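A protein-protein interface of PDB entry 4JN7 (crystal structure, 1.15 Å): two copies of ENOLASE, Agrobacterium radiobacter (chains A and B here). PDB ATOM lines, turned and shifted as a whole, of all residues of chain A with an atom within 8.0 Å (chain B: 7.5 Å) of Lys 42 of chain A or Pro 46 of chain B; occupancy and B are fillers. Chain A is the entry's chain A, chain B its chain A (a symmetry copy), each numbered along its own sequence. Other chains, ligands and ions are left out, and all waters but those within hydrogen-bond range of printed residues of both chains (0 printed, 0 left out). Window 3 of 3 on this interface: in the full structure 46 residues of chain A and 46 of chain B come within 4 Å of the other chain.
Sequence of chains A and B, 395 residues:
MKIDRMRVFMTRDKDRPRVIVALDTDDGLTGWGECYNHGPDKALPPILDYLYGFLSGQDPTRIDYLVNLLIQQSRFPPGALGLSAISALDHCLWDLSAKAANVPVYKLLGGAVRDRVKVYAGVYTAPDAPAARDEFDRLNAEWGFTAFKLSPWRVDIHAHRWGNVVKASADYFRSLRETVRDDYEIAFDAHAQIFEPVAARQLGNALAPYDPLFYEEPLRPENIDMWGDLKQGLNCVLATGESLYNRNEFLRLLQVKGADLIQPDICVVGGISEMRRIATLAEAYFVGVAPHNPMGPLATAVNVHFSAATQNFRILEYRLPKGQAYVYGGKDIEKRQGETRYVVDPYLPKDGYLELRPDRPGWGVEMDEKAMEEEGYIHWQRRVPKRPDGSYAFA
Of the printed residues of chain B, Pro 40 of chain A touches Tyr 50 (3.7 Å).
Of chain B, only Pro 46 (3.7 Å) comes within 4 Å of Lys 42 of chain A.
Of the printed residues of chain B, Ile 47 of chain A touches Ala 43 (3.6 Å).
Printed residues of chain B within 4 Å of His 379 of chain A: Tyr 50 (3.6 Å).
Printed residues of chain A within 4 Å of Ala 43 of chain B: Ala 43 (3.7 Å), Pro 46 (3.7 Å) and Ile 47 (3.6 Å).
Leu 44 of chain B touches none of the printed residues of chain A.
Of chain A, only Lys 42 and Ala 43 come within 4 Å of Pro 46 of chain B.
Of the printed residues of chain A, Tyr 50 of chain B touches Gly 39 (3.6 Å), Pro 40 (3.7 Å) and His 379 (3.6 Å).
Leu 51 of chain B touches none of the printed residues of chain A.
The nearest residue of chain A that does not touch Pro 46 of chain B is Pro 40 of chain A (4.2 Å).
The nearest printed residue of chain B that does not touch His 379 of chain A is Asp 49 of chain B (6.9 Å).
Lys 42 of chain A touches Pro 46 of chain B, and with the chains exchanged Pro 46 of chain A touches Lys 42 of chain B.
Ala 43 of chain B touches its own counterpart, Ala 43 of chain A.
Ala 43 of chain A touches Pro 46 of chain B, and with the chains exchanged Pro 46 of chain A touches Ala 43 of chain B.
Ala 43 of chain A touches Ile 47 of chain B, and with the chains exchanged Ile 47 of chain A touches Ala 43 of chain B.
Positions printed for both chains: 41, 42, 43, 44, 45, 46 and 47.
Of the 11 pairs that touch across the chains among the printed residues, 7 have their exchanged pair printed and touching as well.
The backbone NH of Gly 39 of chain A sits close to the side-chain amide nitrogen of Asn 37 of chain A (3.4 Å).
N of Gly 39 of chain A is in hydrogen-bond range of OD1 of Asp 41 of chain A.
Of the 15 printed residues of chain B, 5 touch a printed residue of chain A.
Of the 17 printed residues of chain A, 8 touch a printed residue of chain B.
Hydrophobic or aromatic side chains of chain A that line the printed part of chain B: Pro 40, Ala 43, Pro 46, Ile 47, Leu 81 and His 379.
Among the printed residues, 11 pairs touch across the chains.
Among the printed residues, pairs that only touch across the chains: Leu 81 of chain A with Ile 47 of chain B (3.4 Å), Ala 43 of chain A with Ile 47 of chain B (3.6 Å), Ile 47 of chain A with Ala 43 of chain B (3.6 Å), Gly 39 of chain A with Tyr 50 of chain B (3.6 Å), His 379 of chain A with Tyr 50 of chain B (3.6 Å), Pro 40 of chain A with Tyr 50 of chain B (3.7 Å), Ala 43 of chain A with Ala 43 of chain B (3.7 Å), Pro 46 of chain A with Lys 42 of chain B (3.7 Å), Lys 42 of chain A with Pro 46 of chain B (3.7 Å), Ala 43 of chain A with Pro 46 of chain B (3.7 Å) and Pro 46 of chain A with Ala 43 of chain B (3.7 Å).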
ATOM      1  N   MET A  10      20.680 -11.396   5.428  1.00  0.00           N
ATOM      2  CA  MET A  10      19.961 -10.678   4.395  1.00  0.00           C
ATOM      3  C   MET A  10      20.962 -10.307   3.328  1.00  0.00           C
ATOM      4  O   MET A  10      21.822  -9.451   3.541  1.00  0.00           O
ATOM      5  CB  MET A  10      19.291  -9.418   4.945  1.00  0.00           C
ATOM      6  CG  MET A  10      18.632  -8.588   3.857  1.00  0.00           C
ATOM      7  SD  MET A  10      17.267  -9.446   3.046  1.00  0.00           S
ATOM      8  CE  MET A  10      16.016  -9.279   4.321  1.00  0.00           C
ATOM      9  N   PRO A  17      16.469  -9.460  -3.562  1.00  0.00           N
ATOM     10  CA  PRO A  17      17.012  -9.790  -2.245  1.00  0.00           C
ATOM     11  C   PRO A  17      16.892 -11.288  -1.968  1.00  0.00           C
ATOM     12  O   PRO A  17      16.128 -11.996  -2.624  1.00  0.00           O
ATOM     13  CB  PRO A  17      16.137  -8.981  -1.297  1.00  0.00           C
ATOM     14  CG  PRO A  17      14.806  -8.914  -2.000  1.00  0.00           C
ATOM     15  CD  PRO A  17      15.158  -8.799  -3.467  1.00  0.00           C
ATOM     16  N   VAL A  19      17.154 -14.062   1.515  1.00  0.00           N
ATOM     17  CA  VAL A  19      17.399 -14.418   2.903  1.00  0.00           C
ATOM     18  C   VAL A  19      17.920 -15.845   2.970  1.00  0.00           C
ATOM     19  O   VAL A  19      17.282 -16.789   2.471  1.00  0.00           O
ATOM     20  CB  VAL A  19      16.134 -14.221   3.754  1.00  0.00           C
ATOM     21  CG1 VAL A  19      16.373 -14.674   5.179  1.00  0.00           C
ATOM     22  CG2 VAL A  19      15.728 -12.757   3.729  1.00  0.00           C
ATOM     23  N   ASN A  37      12.163 -15.396  -2.597  1.00  0.00           N
ATOM     24  CA  ASN A  37      11.971 -13.944  -2.577  1.00  0.00           C
ATOM     25  C   ASN A  37      10.577 -13.558  -3.084  1.00  0.00           C
ATOM     26  O   ASN A  37      10.369 -13.305  -4.268  1.00  0.00           O
ATOM     27  CB  ASN A  37      13.055 -13.257  -3.427  1.00  0.00           C
ATOM     28  CG  ASN A  37      12.746 -11.792  -3.719  1.00  0.00           C
ATOM     29  OD1 ASN A  37      12.930 -11.320  -4.839  1.00  0.00           O
ATOM     30  ND2 ASN A  37      12.269 -11.075  -2.721  1.00  0.00           N
ATOM     31  N   GLY A  39       8.940 -10.810  -1.980  1.00  0.00           N
ATOM     32  CA  GLY A  39       8.945  -9.376  -2.184  1.00  0.00           C
ATOM     33  C   GLY A  39       9.430  -8.657  -0.946  1.00  0.00           C
ATOM     34  O   GLY A  39      10.568  -8.185  -0.892  1.00  0.00           O
ATOM     35  N   PRO A  40       8.568  -8.578   0.078  1.00  0.00           N
ATOM     36  CA  PRO A  40       8.894  -7.874   1.323  1.00  0.00           C
ATOM     37  C   PRO A  40       9.790  -8.709   2.220  1.00  0.00           C
ATOM     38  O   PRO A  40       9.392  -9.147   3.310  1.00  0.00           O
ATOM     39  CB  PRO A  40       7.526  -7.679   1.960  1.00  0.00           C
ATOM     40  CG  PRO A  40       6.754  -8.876   1.506  1.00  0.00           C
ATOM     41  CD  PRO A  40       7.195  -9.115   0.090  1.00  0.00           C
ATOM     42  N   ASP A  41      11.005  -8.956   1.779  1.00  0.00           N
ATOM     43  CA  ASP A  41      11.826  -9.940   2.461  1.00  0.00           C
ATOM     44  C   ASP A  41      12.322  -9.499   3.852  1.00  0.00           C
ATOM     45  O   ASP A  41      12.752 -10.334   4.646  1.00  0.00           O
ATOM     46  CB  ASP A  41      12.923 -10.444   1.523  1.00  0.00           C
ATOM     47  CG  ASP A  41      12.357 -11.360   0.404  1.00  0.00           C
ATOM     48  OD1 ASP A  41      11.131 -11.327   0.142  1.00  0.00           O
ATOM     49  OD2 ASP A  41      13.135 -12.118  -0.184  1.00  0.00           O
ATOM     50  N   LYS A  42      12.212  -8.219   4.184  1.00  0.00           N
ATOM     51  CA  LYS A  42      12.464  -7.805   5.556  1.00  0.00           C
ATOM     52  C   LYS A  42      11.467  -8.425   6.534  1.00  0.00           C
ATOM     53  O   LYS A  42      11.699  -8.379   7.738  1.00  0.00           O
ATOM     54  CB  LYS A  42      12.485  -6.278   5.678  1.00  0.00           C
ATOM     55  CG  LYS A  42      13.711  -5.634   5.036  1.00  0.00           C
ATOM     56  CD  LYS A  42      13.645  -4.120   5.117  1.00  0.00           C
ATOM     57  CE  LYS A  42      14.814  -3.480   4.399  1.00  0.00           C
ATOM     58  NZ  LYS A  42      14.786  -1.993   4.513  1.00  0.00           N
ATOM     59  N   ALA A  43      10.381  -9.009   6.042  1.00  0.00           N
ATOM     60  CA  ALA A  43       9.452  -9.714   6.913  1.00  0.00           C
ATOM     61  C   ALA A  43       9.992 -11.085   7.328  1.00  0.00           C
ATOM     62  O   ALA A  43       9.524 -11.671   8.312  1.00  0.00           O
ATOM     63  CB  ALA A  43       8.106  -9.862   6.235  1.00  0.00           C
ATOM     64  N   LEU A  44      10.952 -11.624   6.583  1.00  0.00           N
ATOM     65  CA  LEU A  44      11.391 -12.988   6.845  1.00  0.00           C
ATOM     66  C   LEU A  44      12.159 -13.148   8.168  1.00  0.00           C
ATOM     67  O   LEU A  44      11.887 -14.088   8.900  1.00  0.00           O
ATOM     68  CB  LEU A  44      12.173 -13.561   5.657  1.00  0.00           C
ATOM     69  CG  LEU A  44      11.336 -13.772   4.395  1.00  0.00           C
ATOM     70  CD1 LEU A  44      12.240 -14.032   3.197  1.00  0.00           C
ATOM     71  CD2 LEU A  44      10.349 -14.919   4.555  1.00  0.00           C
ATOM     72  N   PRO A  45      13.100 -12.245   8.488  1.00  0.00           N
ATOM     73  CA  PRO A  45      13.798 -12.442   9.763  1.00  0.00           C
ATOM     74  C   PRO A  45      12.863 -12.507  10.996  1.00  0.00           C
ATOM     75  O   PRO A  45      13.058 -13.397  11.827  1.00  0.00           O
ATOM     76  CB  PRO A  45      14.782 -11.267   9.796  1.00  0.00           C
ATOM     77  CG  PRO A  45      15.083 -11.012   8.320  1.00  0.00           C
ATOM     78  CD  PRO A  45      13.734 -11.191   7.666  1.00  0.00           C
ATOM     79  N   PRO A  46      11.855 -11.615  11.113  1.00  0.00           N
ATOM     80  CA  PRO A  46      10.981 -11.794  12.286  1.00  0.00           C
ATOM     81  C   PRO A  46      10.145 -13.075  12.254  1.00  0.00           C
ATOM     82  O   PRO A  46       9.827 -13.619  13.310  1.00  0.00           O
ATOM     83  CB  PRO A  46      10.069 -10.560  12.266  1.00  0.00           C
ATOM     84  CG  PRO A  46      10.266  -9.923  10.930  1.00  0.00           C
ATOM     85  CD  PRO A  46      11.638 -10.313  10.457  1.00  0.00           C
ATOM     86  N   ILE A  47       9.769 -13.551  11.071  1.00  0.00           N
ATOM     87  CA  ILE A  47       9.088 -14.840  10.991  1.00  0.00           C
ATOM     88  C   ILE A  47      10.021 -15.936  11.480  1.00  0.00           C
ATOM     89  O   ILE A  47       9.648 -16.770  12.306  1.00  0.00           O
ATOM     90  CB  ILE A  47       8.599 -15.165   9.564  1.00  0.00           C
ATOM     91  CG1 ILE A  47       7.573 -14.127   9.106  1.00  0.00           C
ATOM     92  CG2 ILE A  47       8.002 -16.546   9.529  1.00  0.00           C
ATOM     93  CD1 ILE A  47       7.306 -14.167   7.621  1.00  0.00           C
ATOM     94  N   LEU A  81       4.741 -15.959   2.684  1.00  0.00           N
ATOM     95  CA  LEU A  81       5.881 -15.577   3.508  1.00  0.00           C
ATOM     96  C   LEU A  81       6.200 -16.639   4.553  1.00  0.00           C
ATOM     97  O   LEU A  81       7.355 -17.009   4.741  1.00  0.00           O
ATOM     98  CB  LEU A  81       5.631 -14.211   4.136  1.00  0.00           C
ATOM     99  CG  LEU A  81       5.619 -13.070   3.114  1.00  0.00           C
ATOM    100  CD1 LEU A  81       5.082 -11.796   3.748  1.00  0.00           C
ATOM    101  CD2 LEU A  81       6.996 -12.827   2.515  1.00  0.00           C
ATOM    102  N   TYR A 377      20.365  -6.155   1.577  1.00  0.00           N
ATOM    103  CA  TYR A 377      19.048  -6.005   0.976  1.00  0.00           C
ATOM    104  C   TYR A 377      19.073  -5.085  -0.236  1.00  0.00           C
ATOM    105  O   TYR A 377      19.805  -4.104  -0.284  1.00  0.00           O
ATOM    106  CB  TYR A 377      18.101  -5.411   2.008  1.00  0.00           C
ATOM    107  CG  TYR A 377      16.664  -5.256   1.569  1.00  0.00           C
ATOM    108  CD1 TYR A 377      15.803  -6.336   1.579  1.00  0.00           C
ATOM    109  CD2 TYR A 377      16.154  -4.018   1.187  1.00  0.00           C
ATOM    110  CE1 TYR A 377      14.482  -6.200   1.215  1.00  0.00           C
ATOM    111  CE2 TYR A 377      14.829  -3.873   0.813  1.00  0.00           C
ATOM    112  CZ  TYR A 377      13.999  -4.973   0.843  1.00  0.00           C
ATOM    113  OH  TYR A 377      12.682  -4.866   0.499  1.00  0.00           O
ATOM    114  N   ILE A 378      18.238  -5.423  -1.207  1.00  0.00           N
ATOM    115  CA  ILE A 378      17.915  -4.546  -2.312  1.00  0.00           C
ATOM    116  C   ILE A 378      16.407  -4.662  -2.530  1.00  0.00           C
ATOM    117  O   ILE A 378      15.845  -5.761  -2.472  1.00  0.00           O
ATOM    118  CB  ILE A 378      18.695  -4.940  -3.590  1.00  0.00           C
ATOM    119  CG1 ILE A 378      18.390  -3.962  -4.725  1.00  0.00           C
ATOM    120  CG2 ILE A 378      18.370  -6.362  -4.026  1.00  0.00           C
ATOM    121  CD1 ILE A 378      19.275  -4.143  -5.948  1.00  0.00           C
ATOM    122  N   HIS A 379      15.733  -3.541  -2.741  1.00  0.00           N
ATOM    123  CA  HIS A 379      14.294  -3.550  -3.001  1.00  0.00           C
ATOM    124  C   HIS A 379      13.996  -4.110  -4.384  1.00  0.00           C
ATOM    125  O   HIS A 379      14.618  -3.705  -5.371  1.00  0.00           O
ATOM    126  CB  HIS A 379      13.727  -2.131  -2.905  1.00  0.00           C
ATOM    127  CG  HIS A 379      12.284  -2.037  -3.297  1.00  0.00           C
ATOM    128  ND1 HIS A 379      11.253  -2.193  -2.396  1.00  0.00           N
ATOM    129  CD2 HIS A 379      11.700  -1.833  -4.502  1.00  0.00           C
ATOM    130  CE1 HIS A 379      10.098  -2.068  -3.026  1.00  0.00           C
ATOM    131  NE2 HIS A 379      10.341  -1.860  -4.306  1.00  0.00           N
ATOM    132  N   MET B   6       1.467   6.543   6.227  1.00  0.00           N
ATOM    133  CA  MET B   6       0.986   5.371   6.943  1.00  0.00           C
ATOM    134  C   MET B   6       1.619   5.371   8.329  1.00  0.00           C
ATOM    135  O   MET B   6       2.811   5.655   8.479  1.00  0.00           O
ATOM    136  CB  MET B   6       1.367   4.091   6.191  1.00  0.00           C
ATOM    137  CG  MET B   6       0.942   2.815   6.916  1.00  0.00           C
ATOM    138  SD  MET B   6       1.411   1.291   6.061  1.00  0.00           S
ATOM    139  CE  MET B   6       3.187   1.399   6.206  1.00  0.00           C
ATOM    140  N   VAL B   8       1.881   2.786  11.731  1.00  0.00           N
ATOM    141  CA  VAL B   8       1.666   1.407  12.146  1.00  0.00           C
ATOM    142  C   VAL B   8       1.914   1.332  13.643  1.00  0.00           C
ATOM    143  O   VAL B   8       2.950   1.799  14.142  1.00  0.00           O
ATOM    144  CB  VAL B   8       2.609   0.452  11.411  1.00  0.00           C
ATOM    145  CG1 VAL B   8       2.406  -0.966  11.897  1.00  0.00           C
ATOM    146  CG2 VAL B   8       2.389   0.537   9.904  1.00  0.00           C
ATOM    147  N   ASP B  41       3.827 -11.393  14.673  1.00  0.00           N
ATOM    148  CA  ASP B  41       3.297 -10.126  14.206  1.00  0.00           C
ATOM    149  C   ASP B  41       4.364  -9.037  13.974  1.00  0.00           C
ATOM    150  O   ASP B  41       4.095  -8.045  13.299  1.00  0.00           O
ATOM    151  CB  ASP B  41       2.127  -9.692  15.090  1.00  0.00           C
ATOM    152  CG  ASP B  41       0.864 -10.566  14.853  1.00  0.00           C
ATOM    153  OD1 ASP B  41       0.983 -11.682  14.294  1.00  0.00           O
ATOM    154  OD2 ASP B  41      -0.233 -10.120  15.205  1.00  0.00           O
ATOM    155  N   LYS B  42       5.582  -9.233  14.464  1.00  0.00           N
ATOM    156  CA  LYS B  42       6.665  -8.341  14.083  1.00  0.00           C
ATOM    157  C   LYS B  42       6.961  -8.406  12.584  1.00  0.00           C
ATOM    158  O   LYS B  42       7.663  -7.539  12.072  1.00  0.00           O
ATOM    159  CB  LYS B  42       7.924  -8.615  14.910  1.00  0.00           C
ATOM    160  CG  LYS B  42       7.800  -8.182  16.369  1.00  0.00           C
ATOM    161  CD  LYS B  42       9.043  -8.545  17.160  1.00  0.00           C
ATOM    162  CE  LYS B  42       8.880  -8.199  18.625  1.00  0.00           C
ATOM    163  NZ  LYS B  42      10.114  -8.507  19.406  1.00  0.00           N
ATOM    164  N   ALA B  43       6.434  -9.401  11.880  1.00  0.00           N
ATOM    165  CA  ALA B  43       6.587  -9.455  10.434  1.00  0.00           C
ATOM    166  C   ALA B  43       5.654  -8.469   9.727  1.00  0.00           C
ATOM    167  O   ALA B  43       5.874  -8.126   8.559  1.00  0.00           O
ATOM    168  CB  ALA B  43       6.343 -10.862   9.932  1.00  0.00           C
ATOM    169  N   LEU B  44       4.598  -8.023  10.400  1.00  0.00           N
ATOM    170  CA  LEU B  44       3.600  -7.206   9.725  1.00  0.00           C
ATOM    171  C   LEU B  44       4.102  -5.804   9.343  1.00  0.00           C
ATOM    172  O   LEU B  44       3.857  -5.370   8.228  1.00  0.00           O
ATOM    173  CB  LEU B  44       2.292  -7.149  10.522  1.00  0.00           C
ATOM    174  CG  LEU B  44       1.550  -8.483  10.613  1.00  0.00           C
ATOM    175  CD1 LEU B  44       0.455  -8.409  11.669  1.00  0.00           C
ATOM    176  CD2 LEU B  44       0.949  -8.888   9.275  1.00  0.00           C
ATOM    177  N   PRO B  45       4.806  -5.097  10.243  1.00  0.00           N
ATOM    178  CA  PRO B  45       5.265  -3.768   9.826  1.00  0.00           C
ATOM    179  C   PRO B  45       6.133  -3.769   8.543  1.00  0.00           C
ATOM    180  O   PRO B  45       5.890  -2.925   7.677  1.00  0.00           O
ATOM    181  CB  PRO B  45       6.003  -3.259  11.070  1.00  0.00           C
ATOM    182  CG  PRO B  45       5.268  -3.939  12.225  1.00  0.00           C
ATOM    183  CD  PRO B  45       5.014  -5.328  11.690  1.00  0.00           C
ATOM    184  N   PRO B  46       7.102  -4.699   8.398  1.00  0.00           N
ATOM    185  CA  PRO B  46       7.833  -4.660   7.119  1.00  0.00           C
ATOM    186  C   PRO B  46       6.984  -5.028   5.900  1.00  0.00           C
ATOM    187  O   PRO B  46       7.248  -4.536   4.805  1.00  0.00           O
ATOM    188  CB  PRO B  46       8.969  -5.674   7.304  1.00  0.00           C
ATOM    189  CG  PRO B  46       8.636  -6.445   8.540  1.00  0.00           C
ATOM    190  CD  PRO B  46       7.774  -5.556   9.391  1.00  0.00           C
ATOM    191  N   ILE B  47       5.989  -5.893   6.067  1.00  0.00           N
ATOM    192  CA  ILE B  47       5.073  -6.167   4.963  1.00  0.00           C
ATOM    193  C   ILE B  47       4.318  -4.897   4.606  1.00  0.00           C
ATOM    194  O   ILE B  47       4.231  -4.512   3.439  1.00  0.00           O
ATOM    195  CB  ILE B  47       4.074  -7.297   5.287  1.00  0.00           C
ATOM    196  CG1 ILE B  47       4.821  -8.608   5.537  1.00  0.00           C
ATOM    197  CG2 ILE B  47       3.096  -7.456   4.153  1.00  0.00           C
ATOM    198  CD1 ILE B  47       3.965  -9.667   6.190  1.00  0.00           C
ATOM    199  N   LEU B  48       3.780  -4.236   5.625  1.00  0.00           N
ATOM    200  CA  LEU B  48       3.041  -2.993   5.426  1.00  0.00           C
ATOM    201  C   LEU B  48       3.899  -1.916   4.756  1.00  0.00           C
ATOM    202  O   LEU B  48       3.423  -1.201   3.869  1.00  0.00           O
ATOM    203  CB  LEU B  48       2.470  -2.491   6.759  1.00  0.00           C
ATOM    204  CG  LEU B  48       1.338  -3.368   7.316  1.00  0.00           C
ATOM    205  CD1 LEU B  48       1.170  -3.182   8.808  1.00  0.00           C
ATOM    206  CD2 LEU B  48       0.018  -3.108   6.593  1.00  0.00           C
ATOM    207  N   ASP B  49       5.156  -1.797   5.172  1.00  0.00           N
ATOM    208  CA  ASP B  49       6.061  -0.828   4.569  1.00  0.00           C
ATOM    209  C   ASP B  49       6.178  -1.064   3.061  1.00  0.00           C
ATOM    210  O   ASP B  49       6.208  -0.121   2.266  1.00  0.00           O
ATOM    211  CB  ASP B  49       7.458  -0.947   5.180  1.00  0.00           C
ATOM    212  CG  ASP B  49       7.546  -0.402   6.588  1.00  0.00           C
ATOM    213  OD1 ASP B  49       6.686   0.410   6.991  1.00  0.00           O
ATOM    214  OD2 ASP B  49       8.513  -0.786   7.285  1.00  0.00           O
ATOM    215  N   TYR B  50       6.301  -2.326   2.667  1.00  0.00           N
ATOM    216  CA  TYR B  50       6.441  -2.702   1.266  1.00  0.00           C
ATOM    217  C   TYR B  50       5.146  -2.409   0.507  1.00  0.00           C
ATOM    218  O   TYR B  50       5.157  -1.802  -0.570  1.00  0.00           O
ATOM    219  CB  TYR B  50       6.819  -4.179   1.193  1.00  0.00           C
ATOM    220  CG  TYR B  50       7.132  -4.730  -0.169  1.00  0.00           C
ATOM    221  CD1 TYR B  50       8.418  -4.668  -0.693  1.00  0.00           C
ATOM    222  CD2 TYR B  50       6.143  -5.356  -0.915  1.00  0.00           C
ATOM    223  CE1 TYR B  50       8.708  -5.209  -1.931  1.00  0.00           C
ATOM    224  CE2 TYR B  50       6.422  -5.891  -2.151  1.00  0.00           C
ATOM    225  CZ  TYR B  50       7.699  -5.806  -2.656  1.00  0.00           C
ATOM    226  OH  TYR B  50       7.918  -6.374  -3.894  1.00  0.00           O
ATOM    227  N   LEU B  51       4.020  -2.810   1.078  1.00  0.00           N
ATOM    228  CA  LEU B  51       2.743  -2.588   0.413  1.00  0.00           C
ATOM    229  C   LEU B  51       2.432  -1.101   0.259  1.00  0.00           C
ATOM    230  O   LEU B  51       1.822  -0.678  -0.726  1.00  0.00           O
ATOM    231  CB  LEU B  51       1.626  -3.277   1.198  1.00  0.00           C
ATOM    232  CG  LEU B  51       1.718  -4.798   1.227  1.00  0.00           C
ATOM    233  CD1 LEU B  51       0.625  -5.396   2.106  1.00  0.00           C
ATOM    234  CD2 LEU B  51       1.644  -5.384  -0.180  1.00  0.00           C
ATOM    235  N   TYR B  52       2.854  -0.307   1.233  1.00  0.00           N
ATOM    236  CA  TYR B  52       2.575   1.126   1.203  1.00  0.00           C
ATOM    237  C   TYR B  52       3.171   1.800  -0.027  1.00  0.00           C
ATOM    238  O   TYR B  52       2.645   2.794  -0.506  1.00  0.00           O
ATOM    239  CB  TYR B  52       3.040   1.818   2.491  1.00  0.00           C
ATOM    240  CG  TYR B  52       2.764   3.300   2.454  1.00  0.00           C
ATOM    241  CD1 TYR B  52       1.475   3.786   2.627  1.00  0.00           C
ATOM    242  CD2 TYR B  52       3.776   4.206   2.178  1.00  0.00           C
ATOM    243  CE1 TYR B  52       1.206   5.137   2.547  1.00  0.00           C
ATOM    244  CE2 TYR B  52       3.515   5.565   2.111  1.00  0.00           C
ATOM    245  CZ  TYR B  52       2.224   6.014   2.298  1.00  0.00           C
ATOM    246  OH  TYR B  52       1.951   7.358   2.210  1.00  0.00           O
ATOM    247  N   ALA B  85      -1.987  -8.210   6.451  1.00  0.00           N
ATOM    248  CA  ALA B  85      -1.557  -6.844   6.172  1.00  0.00           C
ATOM    249  C   ALA B  85      -2.477  -6.183   5.139  1.00  0.00           C
ATOM    250  O   ALA B  85      -2.917  -5.036   5.318  1.00  0.00           O
ATOM    251  CB  ALA B  85      -0.136  -6.849   5.686  1.00  0.00           C
